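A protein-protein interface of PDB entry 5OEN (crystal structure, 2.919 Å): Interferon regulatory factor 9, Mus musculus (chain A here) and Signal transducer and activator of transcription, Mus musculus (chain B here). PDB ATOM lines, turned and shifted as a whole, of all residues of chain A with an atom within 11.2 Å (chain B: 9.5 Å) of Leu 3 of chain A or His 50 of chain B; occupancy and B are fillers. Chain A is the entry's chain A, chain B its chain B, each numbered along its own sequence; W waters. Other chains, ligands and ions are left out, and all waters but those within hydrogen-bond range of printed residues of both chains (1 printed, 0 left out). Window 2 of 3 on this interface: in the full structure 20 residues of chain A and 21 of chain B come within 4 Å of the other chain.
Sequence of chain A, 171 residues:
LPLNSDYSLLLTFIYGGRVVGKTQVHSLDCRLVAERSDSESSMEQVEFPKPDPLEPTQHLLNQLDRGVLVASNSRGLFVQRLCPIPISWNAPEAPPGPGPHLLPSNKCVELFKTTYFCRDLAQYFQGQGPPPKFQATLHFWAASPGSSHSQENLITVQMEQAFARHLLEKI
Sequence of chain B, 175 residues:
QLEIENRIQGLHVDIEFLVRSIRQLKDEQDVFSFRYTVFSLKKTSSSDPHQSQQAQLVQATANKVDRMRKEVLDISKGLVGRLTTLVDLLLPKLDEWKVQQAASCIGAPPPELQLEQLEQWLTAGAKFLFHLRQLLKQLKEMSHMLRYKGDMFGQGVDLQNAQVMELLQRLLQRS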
ATOM      1  N   LEU A   1      -3.581  17.134  17.106  1.00  0.00           N
ATOM      2  CA  LEU A   1      -3.819  17.915  18.313  1.00  0.00           C
ATOM      3  C   LEU A   1      -4.934  17.283  19.147  1.00  0.00           C
ATOM      4  O   LEU A   1      -6.110  17.563  18.916  1.00  0.00           O
ATOM      5  CB  LEU A   1      -4.185  19.355  17.956  1.00  0.00           C
ATOM      6  CG  LEU A   1      -4.233  20.316  19.145  1.00  0.00           C
ATOM      7  CD1 LEU A   1      -2.955  21.137  19.218  1.00  0.00           C
ATOM      8  CD2 LEU A   1      -5.459  21.210  19.067  1.00  0.00           C
ATOM      9  N   PRO A   2      -4.579  16.433  20.109  1.00  0.00           N
ATOM     10  CA  PRO A   2      -5.609  15.782  20.926  1.00  0.00           C
ATOM     11  C   PRO A   2      -6.244  16.750  21.914  1.00  0.00           C
ATOM     12  O   PRO A   2      -5.704  17.813  22.229  1.00  0.00           O
ATOM     13  CB  PRO A   2      -4.845  14.672  21.662  1.00  0.00           C
ATOM     14  CG  PRO A   2      -3.472  14.635  21.049  1.00  0.00           C
ATOM     15  CD  PRO A   2      -3.228  15.986  20.481  1.00  0.00           C
ATOM     16  N   LEU A   3      -7.420  16.357  22.408  1.00  0.00           N
ATOM     17  CA  LEU A   3      -8.033  17.085  23.515  1.00  0.00           C
ATOM     18  C   LEU A   3      -7.128  17.056  24.738  1.00  0.00           C
ATOM     19  O   LEU A   3      -6.908  18.082  25.392  1.00  0.00           O
ATOM     20  CB  LEU A   3      -9.403  16.489  23.846  1.00  0.00           C
ATOM     21  CG  LEU A   3     -10.501  16.622  22.789  1.00  0.00           C
ATOM     22  CD1 LEU A   3     -11.739  15.849  23.222  1.00  0.00           C
ATOM     23  CD2 LEU A   3     -10.848  18.083  22.533  1.00  0.00           C
ATOM     24  N   ASN A   4      -6.584  15.882  25.058  1.00  0.00           N
ATOM     25  CA  ASN A   4      -5.654  15.743  26.169  1.00  0.00           C
ATOM     26  C   ASN A   4      -4.325  16.409  25.836  1.00  0.00           C
ATOM     27  O   ASN A   4      -3.296  15.735  25.726  1.00  0.00           O
ATOM     28  CB  ASN A   4      -5.441  14.265  26.505  1.00  0.00           C
ATOM     29  CG  ASN A   4      -6.709  13.592  26.996  1.00  0.00           C
ATOM     30  OD1 ASN A   4      -7.563  14.227  27.616  1.00  0.00           O
ATOM     31  ND2 ASN A   4      -6.840  12.299  26.719  1.00  0.00           N
ATOM     32  N   SER A   5      -4.339  17.729  25.674  1.00  0.00           N
ATOM     33  CA  SER A   5      -3.147  18.502  25.357  1.00  0.00           C
ATOM     34  C   SER A   5      -2.808  19.398  26.540  1.00  0.00           C
ATOM     35  O   SER A   5      -3.692  20.052  27.102  1.00  0.00           O
ATOM     36  CB  SER A   5      -3.356  19.341  24.095  1.00  0.00           C
ATOM     37  OG  SER A   5      -3.458  18.520  22.945  1.00  0.00           O
ATOM     38  N   ASP A   6      -1.532  19.422  26.913  1.00  0.00           N
ATOM     39  CA  ASP A   6      -1.074  20.153  28.094  1.00  0.00           C
ATOM     40  C   ASP A   6      -0.653  21.553  27.665  1.00  0.00           C
ATOM     41  O   ASP A   6       0.478  21.768  27.220  1.00  0.00           O
ATOM     42  CB  ASP A   6       0.071  19.405  28.770  1.00  0.00           C
ATOM     43  CG  ASP A   6       0.410  19.960  30.145  1.00  0.00           C
ATOM     44  OD1 ASP A   6      -0.320  20.848  30.633  1.00  0.00           O
ATOM     45  OD2 ASP A   6       1.414  19.507  30.736  1.00  0.00           O
ATOM     46  N   TYR A   7      -1.570  22.515  27.795  1.00  0.00           N
ATOM     47  CA  TYR A   7      -1.286  23.912  27.490  1.00  0.00           C
ATOM     48  C   TYR A   7      -0.835  24.696  28.715  1.00  0.00           C
ATOM     49  O   TYR A   7      -1.007  25.921  28.760  1.00  0.00           O
ATOM     50  CB  TYR A   7      -2.514  24.575  26.865  1.00  0.00           C
ATOM     51  CG  TYR A   7      -2.976  23.923  25.584  1.00  0.00           C
ATOM     52  CD1 TYR A   7      -4.158  23.198  25.540  1.00  0.00           C
ATOM     53  CD2 TYR A   7      -2.227  24.026  24.419  1.00  0.00           C
ATOM     54  CE1 TYR A   7      -4.586  22.598  24.372  1.00  0.00           C
ATOM     55  CE2 TYR A   7      -2.645  23.429  23.245  1.00  0.00           C
ATOM     56  CZ  TYR A   7      -3.825  22.715  23.227  1.00  0.00           C
ATOM     57  OH  TYR A   7      -4.244  22.119  22.059  1.00  0.00           O
ATOM     58  N   SER A   8      -0.258  24.025  29.709  1.00  0.00           N
ATOM     59  CA  SER A   8       0.190  24.705  30.914  1.00  0.00           C
ATOM     60  C   SER A   8       1.423  25.552  30.629  1.00  0.00           C
ATOM     61  O   SER A   8       2.275  25.197  29.809  1.00  0.00           O
ATOM     62  CB  SER A   8       0.501  23.689  32.013  1.00  0.00           C
ATOM     63  OG  SER A   8       1.445  22.732  31.564  1.00  0.00           O
ATOM     64  N   HIS A  26      -0.551  25.946  35.995  1.00  0.00           N
ATOM     65  CA  HIS A  26      -1.591  25.144  35.359  1.00  0.00           C
ATOM     66  C   HIS A  26      -2.874  25.925  35.091  1.00  0.00           C
ATOM     67  O   HIS A  26      -3.874  25.318  34.693  1.00  0.00           O
ATOM     68  CB  HIS A  26      -1.912  23.924  36.228  1.00  0.00           C
ATOM     69  CG  HIS A  26      -0.737  23.030  36.472  1.00  0.00           C
ATOM     70  ND1 HIS A  26      -0.155  22.891  37.713  1.00  0.00           N
ATOM     71  CD2 HIS A  26      -0.037  22.228  35.636  1.00  0.00           C
ATOM     72  CE1 HIS A  26       0.854  22.041  37.632  1.00  0.00           C
ATOM     73  NE2 HIS A  26       0.947  21.626  36.381  1.00  0.00           N
ATOM     74  N   SER A  27      -2.877  27.238  35.292  1.00  0.00           N
ATOM     75  CA  SER A  27      -4.068  28.049  35.087  1.00  0.00           C
ATOM     76  C   SER A  27      -4.006  28.755  33.739  1.00  0.00           C
ATOM     77  O   SER A  27      -2.928  28.999  33.192  1.00  0.00           O
ATOM     78  CB  SER A  27      -4.221  29.079  36.207  1.00  0.00           C
ATOM     79  OG  SER A  27      -5.398  29.848  36.032  1.00  0.00           O
ATOM     80  N   LEU A  28      -5.186  29.080  33.204  1.00  0.00           N
ATOM     81  CA  LEU A  28      -5.253  29.786  31.929  1.00  0.00           C
ATOM     82  C   LEU A  28      -4.544  31.129  31.994  1.00  0.00           C
ATOM     83  O   LEU A  28      -4.007  31.597  30.983  1.00  0.00           O
ATOM     84  CB  LEU A  28      -6.712  29.993  31.515  1.00  0.00           C
ATOM     85  CG  LEU A  28      -7.528  28.753  31.154  1.00  0.00           C
ATOM     86  CD1 LEU A  28      -8.963  29.156  30.855  1.00  0.00           C
ATOM     87  CD2 LEU A  28      -6.921  28.023  29.968  1.00  0.00           C
ATOM     88  N   ASP A  29      -4.533  31.764  33.163  1.00  0.00           N
ATOM     89  CA  ASP A  29      -3.971  33.093  33.321  1.00  0.00           C
ATOM     90  C   ASP A  29      -3.047  33.126  34.527  1.00  0.00           C
ATOM     91  O   ASP A  29      -3.072  32.243  35.389  1.00  0.00           O
ATOM     92  CB  ASP A  29      -5.060  34.157  33.503  1.00  0.00           C
ATOM     93  CG  ASP A  29      -5.927  34.333  32.272  1.00  0.00           C
ATOM     94  OD1 ASP A  29      -5.468  34.009  31.157  1.00  0.00           O
ATOM     95  OD2 ASP A  29      -7.074  34.804  32.425  1.00  0.00           O
ATOM     96  N   SER A  72      -2.015  31.630  28.869  1.00  0.00           N
ATOM     97  CA  SER A  72      -1.558  30.393  28.238  1.00  0.00           C
ATOM     98  C   SER A  72      -2.760  29.463  28.104  1.00  0.00           C
ATOM     99  O   SER A  72      -3.177  28.831  29.080  1.00  0.00           O
ATOM    100  CB  SER A  72      -0.440  29.748  29.049  1.00  0.00           C
ATOM    101  OG  SER A  72       0.044  28.584  28.404  1.00  0.00           O
ATOM    102  N   ASN A  73      -3.312  29.381  26.895  1.00  0.00           N
ATOM    103  CA  ASN A  73      -4.487  28.557  26.635  1.00  0.00           C
ATOM    104  C   ASN A  73      -4.272  27.665  25.415  1.00  0.00           C
ATOM    105  O   ASN A  73      -3.131  27.336  25.073  1.00  0.00           O
ATOM    106  CB  ASN A  73      -5.716  29.452  26.447  1.00  0.00           C
ATOM    107  CG  ASN A  73      -5.560  30.424  25.290  1.00  0.00           C
ATOM    108  OD1 ASN A  73      -4.888  30.135  24.300  1.00  0.00           O
ATOM    109  ND2 ASN A  73      -6.183  31.590  25.416  1.00  0.00           N
ATOM    110  N   SER A  74      -5.359  27.267  24.752  1.00  0.00           N
ATOM    111  CA  SER A  74      -5.246  26.378  23.603  1.00  0.00           C
ATOM    112  C   SER A  74      -4.727  27.092  22.360  1.00  0.00           C
ATOM    113  O   SER A  74      -4.185  26.434  21.467  1.00  0.00           O
ATOM    114  CB  SER A  74      -6.606  25.745  23.305  1.00  0.00           C
ATOM    115  OG  SER A  74      -7.571  26.740  23.014  1.00  0.00           O
ATOM    116  N   ARG A  75      -4.873  28.412  22.281  1.00  0.00           N
ATOM    117  CA  ARG A  75      -4.463  29.158  21.098  1.00  0.00           C
ATOM    118  C   ARG A  75      -3.044  29.701  21.195  1.00  0.00           C
ATOM    119  O   ARG A  75      -2.570  30.323  20.239  1.00  0.00           O
ATOM    120  CB  ARG A  75      -5.430  30.315  20.838  1.00  0.00           C
ATOM    121  CG  ARG A  75      -6.813  29.874  20.403  1.00  0.00           C
ATOM    122  CD  ARG A  75      -7.636  31.055  19.920  1.00  0.00           C
ATOM    123  NE  ARG A  75      -7.775  32.085  20.947  1.00  0.00           N
ATOM    124  CZ  ARG A  75      -8.709  32.088  21.893  1.00  0.00           C
ATOM    125  NH1 ARG A  75      -8.750  33.073  22.779  1.00  0.00           N
ATOM    126  NH2 ARG A  75      -9.604  31.110  21.961  1.00  0.00           N
ATOM    127  N   GLY A  76      -2.358  29.492  22.319  1.00  0.00           N
ATOM    128  CA  GLY A  76      -0.979  29.904  22.464  1.00  0.00           C
ATOM    129  C   GLY A  76      -0.802  30.881  23.613  1.00  0.00           C
ATOM    130  O   GLY A  76      -1.572  30.880  24.581  1.00  0.00           O
ATOM    131  N   PHE A  78      -0.275  34.759  25.187  1.00  0.00           N
ATOM    132  CA  PHE A  78      -0.606  36.167  25.064  1.00  0.00           C
ATOM    133  C   PHE A  78      -0.055  36.897  26.278  1.00  0.00           C
ATOM    134  O   PHE A  78       0.001  36.343  27.379  1.00  0.00           O
ATOM    135  CB  PHE A  78      -2.123  36.401  24.967  1.00  0.00           C
ATOM    136  CG  PHE A  78      -2.838  35.431  24.066  1.00  0.00           C
ATOM    137  CD1 PHE A  78      -3.085  34.133  24.481  1.00  0.00           C
ATOM    138  CD2 PHE A  78      -3.279  35.824  22.815  1.00  0.00           C
ATOM    139  CE1 PHE A  78      -3.745  33.243  23.659  1.00  0.00           C
ATOM    140  CE2 PHE A  78      -3.944  34.937  21.989  1.00  0.00           C
ATOM    141  CZ  PHE A  78      -4.177  33.646  22.412  1.00  0.00           C
ATOM    142  N   THR A 114      -0.566  28.125  18.643  1.00  0.00           N
ATOM    143  CA  THR A 114      -0.596  26.681  18.444  1.00  0.00           C
ATOM    144  C   THR A 114      -1.012  26.315  17.026  1.00  0.00           C
ATOM    145  O   THR A 114      -0.547  25.303  16.491  1.00  0.00           O
ATOM    146  CB  THR A 114      -1.550  26.024  19.445  1.00  0.00           C
ATOM    147  OG1 THR A 114      -2.891  26.467  19.200  1.00  0.00           O
ATOM    148  CG2 THR A 114      -1.155  26.376  20.872  1.00  0.00           C
ATOM    149  N   CYS A 118       1.359  23.811  14.836  1.00  0.00           N
ATOM    150  CA  CYS A 118       0.934  22.552  14.231  1.00  0.00           C
ATOM    151  C   CYS A 118       1.151  22.569  12.723  1.00  0.00           C
ATOM    152  O   CYS A 118       1.611  21.577  12.144  1.00  0.00           O
ATOM    153  CB  CYS A 118      -0.536  22.281  14.555  1.00  0.00           C
ATOM    154  SG  CYS A 118      -0.885  22.002  16.309  1.00  0.00           S
ATOM    155  N   GLN A 161       4.994  26.237  26.450  1.00  0.00           N
ATOM    156  CA  GLN A 161       3.883  25.359  26.782  1.00  0.00           C
ATOM    157  C   GLN A 161       4.345  23.907  26.771  1.00  0.00           C
ATOM    158  O   GLN A 161       5.190  23.510  25.965  1.00  0.00           O
ATOM    159  CB  GLN A 161       2.725  25.551  25.802  1.00  0.00           C
ATOM    160  CG  GLN A 161       2.057  26.914  25.905  1.00  0.00           C
ATOM    161  CD  GLN A 161       0.871  27.055  24.972  1.00  0.00           C
ATOM    162  OE1 GLN A 161       1.017  27.004  23.750  1.00  0.00           O
ATOM    163  NE2 GLN A 161      -0.317  27.229  25.545  1.00  0.00           N
ATOM    164  N   PHE A 163       2.942  21.104  25.892  1.00  0.00           N
ATOM    165  CA  PHE A 163       2.680  20.289  24.710  1.00  0.00           C
ATOM    166  C   PHE A 163       3.742  20.495  23.639  1.00  0.00           C
ATOM    167  O   PHE A 163       4.025  19.575  22.863  1.00  0.00           O
ATOM    168  CB  PHE A 163       1.295  20.608  24.144  1.00  0.00           C
ATOM    169  CG  PHE A 163       1.292  21.725  23.131  1.00  0.00           C
ATOM    170  CD1 PHE A 163       1.184  23.044  23.534  1.00  0.00           C
ATOM    171  CD2 PHE A 163       1.394  21.451  21.775  1.00  0.00           C
ATOM    172  CE1 PHE A 163       1.182  24.068  22.606  1.00  0.00           C
ATOM    173  CE2 PHE A 163       1.394  22.470  20.845  1.00  0.00           C
ATOM    174  CZ  PHE A 163       1.287  23.780  21.260  1.00  0.00           C
ATOM    175  N   LEU A 167       6.308  17.345  21.971  1.00  0.00           N
ATOM    176  CA  LEU A 167       6.155  16.835  20.612  1.00  0.00           C
ATOM    177  C   LEU A 167       7.493  16.780  19.884  1.00  0.00           C
ATOM    178  O   LEU A 167       7.754  15.842  19.122  1.00  0.00           O
ATOM    179  CB  LEU A 167       5.166  17.704  19.835  1.00  0.00           C
ATOM    180  CG  LEU A 167       3.703  17.631  20.270  1.00  0.00           C
ATOM    181  CD1 LEU A 167       2.898  18.734  19.599  1.00  0.00           C
ATOM    182  CD2 LEU A 167       3.112  16.268  19.948  1.00  0.00           C
ATOM    183  N   PHE B  39     -10.015  36.510  24.578  1.00  0.00           N
ATOM    184  CA  PHE B  39     -11.141  35.732  24.076  1.00  0.00           C
ATOM    185  C   PHE B  39     -11.548  36.182  22.680  1.00  0.00           C
ATOM    186  O   PHE B  39     -11.947  35.353  21.854  1.00  0.00           O
ATOM    187  CB  PHE B  39     -12.322  35.845  25.041  1.00  0.00           C
ATOM    188  CG  PHE B  39     -13.587  35.220  24.529  1.00  0.00           C
ATOM    189  CD1 PHE B  39     -14.614  36.007  24.044  1.00  0.00           C
ATOM    190  CD2 PHE B  39     -13.748  33.847  24.533  1.00  0.00           C
ATOM    191  CE1 PHE B  39     -15.779  35.437  23.574  1.00  0.00           C
ATOM    192  CE2 PHE B  39     -14.908  33.272  24.063  1.00  0.00           C
ATOM    193  CZ  PHE B  39     -15.925  34.069  23.585  1.00  0.00           C
ATOM    194  N   LYS B  42      -8.450  35.591  17.662  1.00  0.00           N
ATOM    195  CA  LYS B  42      -8.607  34.269  17.063  1.00  0.00           C
ATOM    196  C   LYS B  42      -7.519  34.002  16.025  1.00  0.00           C
ATOM    197  O   LYS B  42      -7.420  34.704  15.019  1.00  0.00           O
ATOM    198  CB  LYS B  42      -9.990  34.143  16.418  1.00  0.00           C
ATOM    199  CG  LYS B  42     -11.153  34.394  17.376  1.00  0.00           C
ATOM    200  CD  LYS B  42     -11.217  33.364  18.500  1.00  0.00           C
ATOM    201  CE  LYS B  42     -11.561  31.979  17.981  1.00  0.00           C
ATOM    202  NZ  LYS B  42     -11.595  30.977  19.078  1.00  0.00           N
ATOM    203  N   SER B  47     -13.537  26.361  15.696  1.00  0.00           N
ATOM    204  CA  SER B  47     -13.220  26.630  17.093  1.00  0.00           C
ATOM    205  C   SER B  47     -12.825  25.350  17.820  1.00  0.00           C
ATOM    206  O   SER B  47     -13.154  24.247  17.383  1.00  0.00           O
ATOM    207  CB  SER B  47     -14.414  27.274  17.799  1.00  0.00           C
ATOM    208  OG  SER B  47     -14.128  27.515  19.166  1.00  0.00           O
ATOM    209  N   ASP B  48     -12.110  25.512  18.936  1.00  0.00           N
ATOM    210  CA  ASP B  48     -11.774  24.393  19.806  1.00  0.00           C
ATOM    211  C   ASP B  48     -12.702  24.396  21.009  1.00  0.00           C
ATOM    212  O   ASP B  48     -12.835  25.439  21.665  1.00  0.00           O
ATOM    213  CB  ASP B  48     -10.325  24.483  20.274  1.00  0.00           C
ATOM    214  CG  ASP B  48      -9.336  24.246  19.151  1.00  0.00           C
ATOM    215  OD1 ASP B  48      -9.732  23.655  18.124  1.00  0.00           O
ATOM    216  OD2 ASP B  48      -8.161  24.644  19.298  1.00  0.00           O
ATOM    217  N   PRO B  49     -13.364  23.275  21.341  1.00  0.00           N
ATOM    218  CA  PRO B  49     -14.263  23.267  22.506  1.00  0.00           C
ATOM    219  C   PRO B  49     -13.641  23.861  23.761  1.00  0.00           C
ATOM    220  O   PRO B  49     -14.361  24.277  24.673  1.00  0.00           O
ATOM    221  CB  PRO B  49     -14.580  21.778  22.682  1.00  0.00           C
ATOM    222  CG  PRO B  49     -14.507  21.229  21.300  1.00  0.00           C
ATOM    223  CD  PRO B  49     -13.416  22.001  20.601  1.00  0.00           C
ATOM    224  N   HIS B  50     -12.307  23.908  23.820  1.00  0.00           N
ATOM    225  CA  HIS B  50     -11.636  24.599  24.914  1.00  0.00           C
ATOM    226  C   HIS B  50     -12.088  26.047  25.044  1.00  0.00           C
ATOM    227  O   HIS B  50     -11.976  26.626  26.130  1.00  0.00           O
ATOM    228  CB  HIS B  50     -10.123  24.556  24.708  1.00  0.00           C
ATOM    229  CG  HIS B  50      -9.472  23.317  25.237  1.00  0.00           C
ATOM    230  ND1 HIS B  50      -9.470  22.120  24.552  1.00  0.00           N
ATOM    231  CD2 HIS B  50      -8.793  23.094  26.386  1.00  0.00           C
ATOM    232  CE1 HIS B  50      -8.820  21.213  25.259  1.00  0.00           C
ATOM    233  NE2 HIS B  50      -8.400  21.778  26.376  1.00  0.00           N
ATOM    234  N   GLN B  51     -12.590  26.647  23.962  1.00  0.00           N
ATOM    235  CA  GLN B  51     -13.021  28.040  24.025  1.00  0.00           C
ATOM    236  C   GLN B  51     -14.175  28.225  24.999  1.00  0.00           C
ATOM    237  O   GLN B  51     -14.337  29.310  25.568  1.00  0.00           O
ATOM    238  CB  GLN B  51     -13.417  28.531  22.631  1.00  0.00           C
ATOM    239  CG  GLN B  51     -13.729  30.016  22.573  1.00  0.00           C
ATOM    240  CD  GLN B  51     -14.068  30.481  21.176  1.00  0.00           C
ATOM    241  OE1 GLN B  51     -14.125  29.683  20.239  1.00  0.00           O
ATOM    242  NE2 GLN B  51     -14.293  31.780  21.025  1.00  0.00           N
ATOM    243  N   SER B  52     -14.995  27.191  25.195  1.00  0.00           N
ATOM    244  CA  SER B  52     -16.031  27.257  26.218  1.00  0.00           C
ATOM    245  C   SER B  52     -15.421  27.613  27.568  1.00  0.00           C
ATOM    246  O   SER B  52     -15.935  28.471  28.294  1.00  0.00           O
ATOM    247  CB  SER B  52     -16.778  25.924  26.294  1.00  0.00           C
ATOM    248  OG  SER B  52     -17.851  25.990  27.218  1.00  0.00           O
ATOM    249  N   GLN B  53     -14.309  26.959  27.914  1.00  0.00           N
ATOM    250  CA  GLN B  53     -13.581  27.314  29.127  1.00  0.00           C
ATOM    251  C   GLN B  53     -13.120  28.765  29.080  1.00  0.00           C
ATOM    252  O   GLN B  53     -13.148  29.467  30.097  1.00  0.00           O
ATOM    253  CB  GLN B  53     -12.387  26.375  29.300  1.00  0.00           C
ATOM    254  CG  GLN B  53     -11.754  26.398  30.679  1.00  0.00           C
ATOM    255  CD  GLN B  53     -10.557  25.472  30.775  1.00  0.00           C
ATOM    256  OE1 GLN B  53     -10.039  25.003  29.760  1.00  0.00           O
ATOM    257  NE2 GLN B  53     -10.113  25.199  31.997  1.00  0.00           N
ATOM    258  N   GLN B  54     -12.695  29.232  27.904  1.00  0.00           N
ATOM    259  CA  GLN B  54     -12.225  30.608  27.771  1.00  0.00           C
ATOM    260  C   GLN B  54     -13.360  31.603  27.989  1.00  0.00           C
ATOM    261  O   GLN B  54     -13.162  32.651  28.613  1.00  0.00           O
ATOM    262  CB  GLN B  54     -11.592  30.810  26.395  1.00  0.00           C
ATOM    263  CG  GLN B  54     -10.900  32.153  26.210  1.00  0.00           C
ATOM    264  CD  GLN B  54      -9.647  32.286  27.053  1.00  0.00           C
ATOM    265  OE1 GLN B  54      -8.949  31.304  27.308  1.00  0.00           O
ATOM    266  NE2 GLN B  54      -9.358  33.505  27.494  1.00  0.00           N
ATOM    267  N   ALA B  55     -14.554  31.296  27.477  1.00  0.00           N
ATOM    268  CA  ALA B  55     -15.690  32.189  27.670  1.00  0.00           C
ATOM    269  C   ALA B  55     -16.167  32.164  29.116  1.00  0.00           C
ATOM    270  O   ALA B  55     -16.460  33.216  29.697  1.00  0.00           O
ATOM    271  CB  ALA B  55     -16.828  31.806  26.724  1.00  0.00           C
ATOM    272  N   GLN B  56     -16.254  30.973  29.714  1.00  0.00           N
ATOM    273  CA  GLN B  56     -16.649  30.876  31.114  1.00  0.00           C
ATOM    274  C   GLN B  56     -15.702  31.660  32.014  1.00  0.00           C
ATOM    275  O   GLN B  56     -16.112  32.141  33.076  1.00  0.00           O
ATOM    276  CB  GLN B  56     -16.698  29.409  31.543  1.00  0.00           C
ATOM    277  CG  GLN B  56     -17.784  28.595  30.848  1.00  0.00           C
ATOM    278  CD  GLN B  56     -17.673  27.108  31.129  1.00  0.00           C
ATOM    279  OE1 GLN B  56     -17.602  26.295  30.206  1.00  0.00           O
ATOM    280  NE2 GLN B  56     -17.665  26.746  32.406  1.00  0.00           N
ATOM    281  N   LEU B  57     -14.438  31.796  31.608  1.00  0.00           N
ATOM    282  CA  LEU B  57     -13.487  32.591  32.378  1.00  0.00           C
ATOM    283  C   LEU B  57     -13.841  34.072  32.313  1.00  0.00           C
ATOM    284  O   LEU B  57     -13.914  34.750  33.345  1.00  0.00           O
ATOM    285  CB  LEU B  57     -12.069  32.354  31.855  1.00  0.00           C
ATOM    286  CG  LEU B  57     -10.927  32.862  32.735  1.00  0.00           C
ATOM    287  CD1 LEU B  57     -10.743  31.958  33.942  1.00  0.00           C
ATOM    288  CD2 LEU B  57      -9.640  32.961  31.933  1.00  0.00           C
HETATM  289  O   HOH W   1      -7.387  34.585  28.807  1.00  0.00           O
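The side-chain amide oxygen of Gln 54 of chain B lies within hydrogen-bond range of the side-chain amide nitrogen of Asn 73 of chain A (3.4 Å).
O of Leu 28 of chain A lies within hydrogen-bond range of N of Ser 72 of chain A (2.9 Å).
OD1 of Asn 73 of chain A lies within hydrogen-bond range of N of Arg 75 of chain A, 2.7 Å away.
O of Asn 73 of chain A lies within hydrogen-bond range of NE2 of Gln 161 of chain A, at 2.9 Å.
The backbone carbonyl oxygen of Ser 74 of chain A sits at hydrogen-bond distance from the side-chain hydroxyl of Thr 114 of chain A (2.6 Å).
O of Arg 75 of chain A lies within hydrogen-bond range of N of Thr 114 of chain A (3.4 Å).
The side-chain amino group (NZ) of Lys 42 of chain B sits at hydrogen-bond distance from the side-chain amide oxygen (OE1) of Gln 51 of chain B.
Among the printed residues, pairs that only touch across the chains: Asp 29 of chain A with Leu 57 of chain B, Arg 75 of chain A with Lys 42 of chain B, Leu 3 of chain A with His 50 of chain B, Ser 74 of chain A with His 50 of chain B, Arg 75 of chain A with Phe 39 of chain B and Leu 28 of chain A with Gln 53 of chain B.
Leu 3 of chain A touches just one residue of chain B: His 50.
Of chain A, only Leu 3 and Ser 74 come within 4 Å of His 50 of chain B.
No residue of chain B comes within 4 Å of Asn 4 of chain A.
No residue of chain A comes within 4 Å of Asp 48 of chain B.
No residue of chain A comes within 4 Å of Ser 52 of chain B.
Of chain A, only Leu 28 (3.9 Å) comes within 4 Å of Gln 53 of chain B.
Printed residues of chain B within 4 Å of Ser 74 of chain A: His 50 (3.8 Å).
Printed residues of chain B within 4 Å of Arg 75 of chain A: Phe 39 (3.8 Å) and Lys 42 (3.5 Å).
Printed residues of chain B within 4 Å of Asp 29 of chain A: Leu 57 (3.2 Å).
Of the printed residues of chain B, Leu 28 of chain A touches Gln 53 (3.9 Å).
Thr 114 of chain A touches none of the printed residues of chain B.
The nearest residue of chain A that does not touch His 50 of chain B is Tyr 7 of chain A (4.4 Å).
The nearest printed residue of chain B that does not touch Ser 74 of chain A is Asp 48 of chain B (4.3 Å).
Of the 23 printed residues of chain A, 6 touch a printed residue of chain B.
Among the printed residues, 7 pairs touch across the chains.
Water W1 lies within hydrogen-bond range of the side-chain amide nitrogen of Gln 54 of chain B (2.6 Å) and the side-chain carboxylate of Asp 29 of chain A (3.1 Å).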
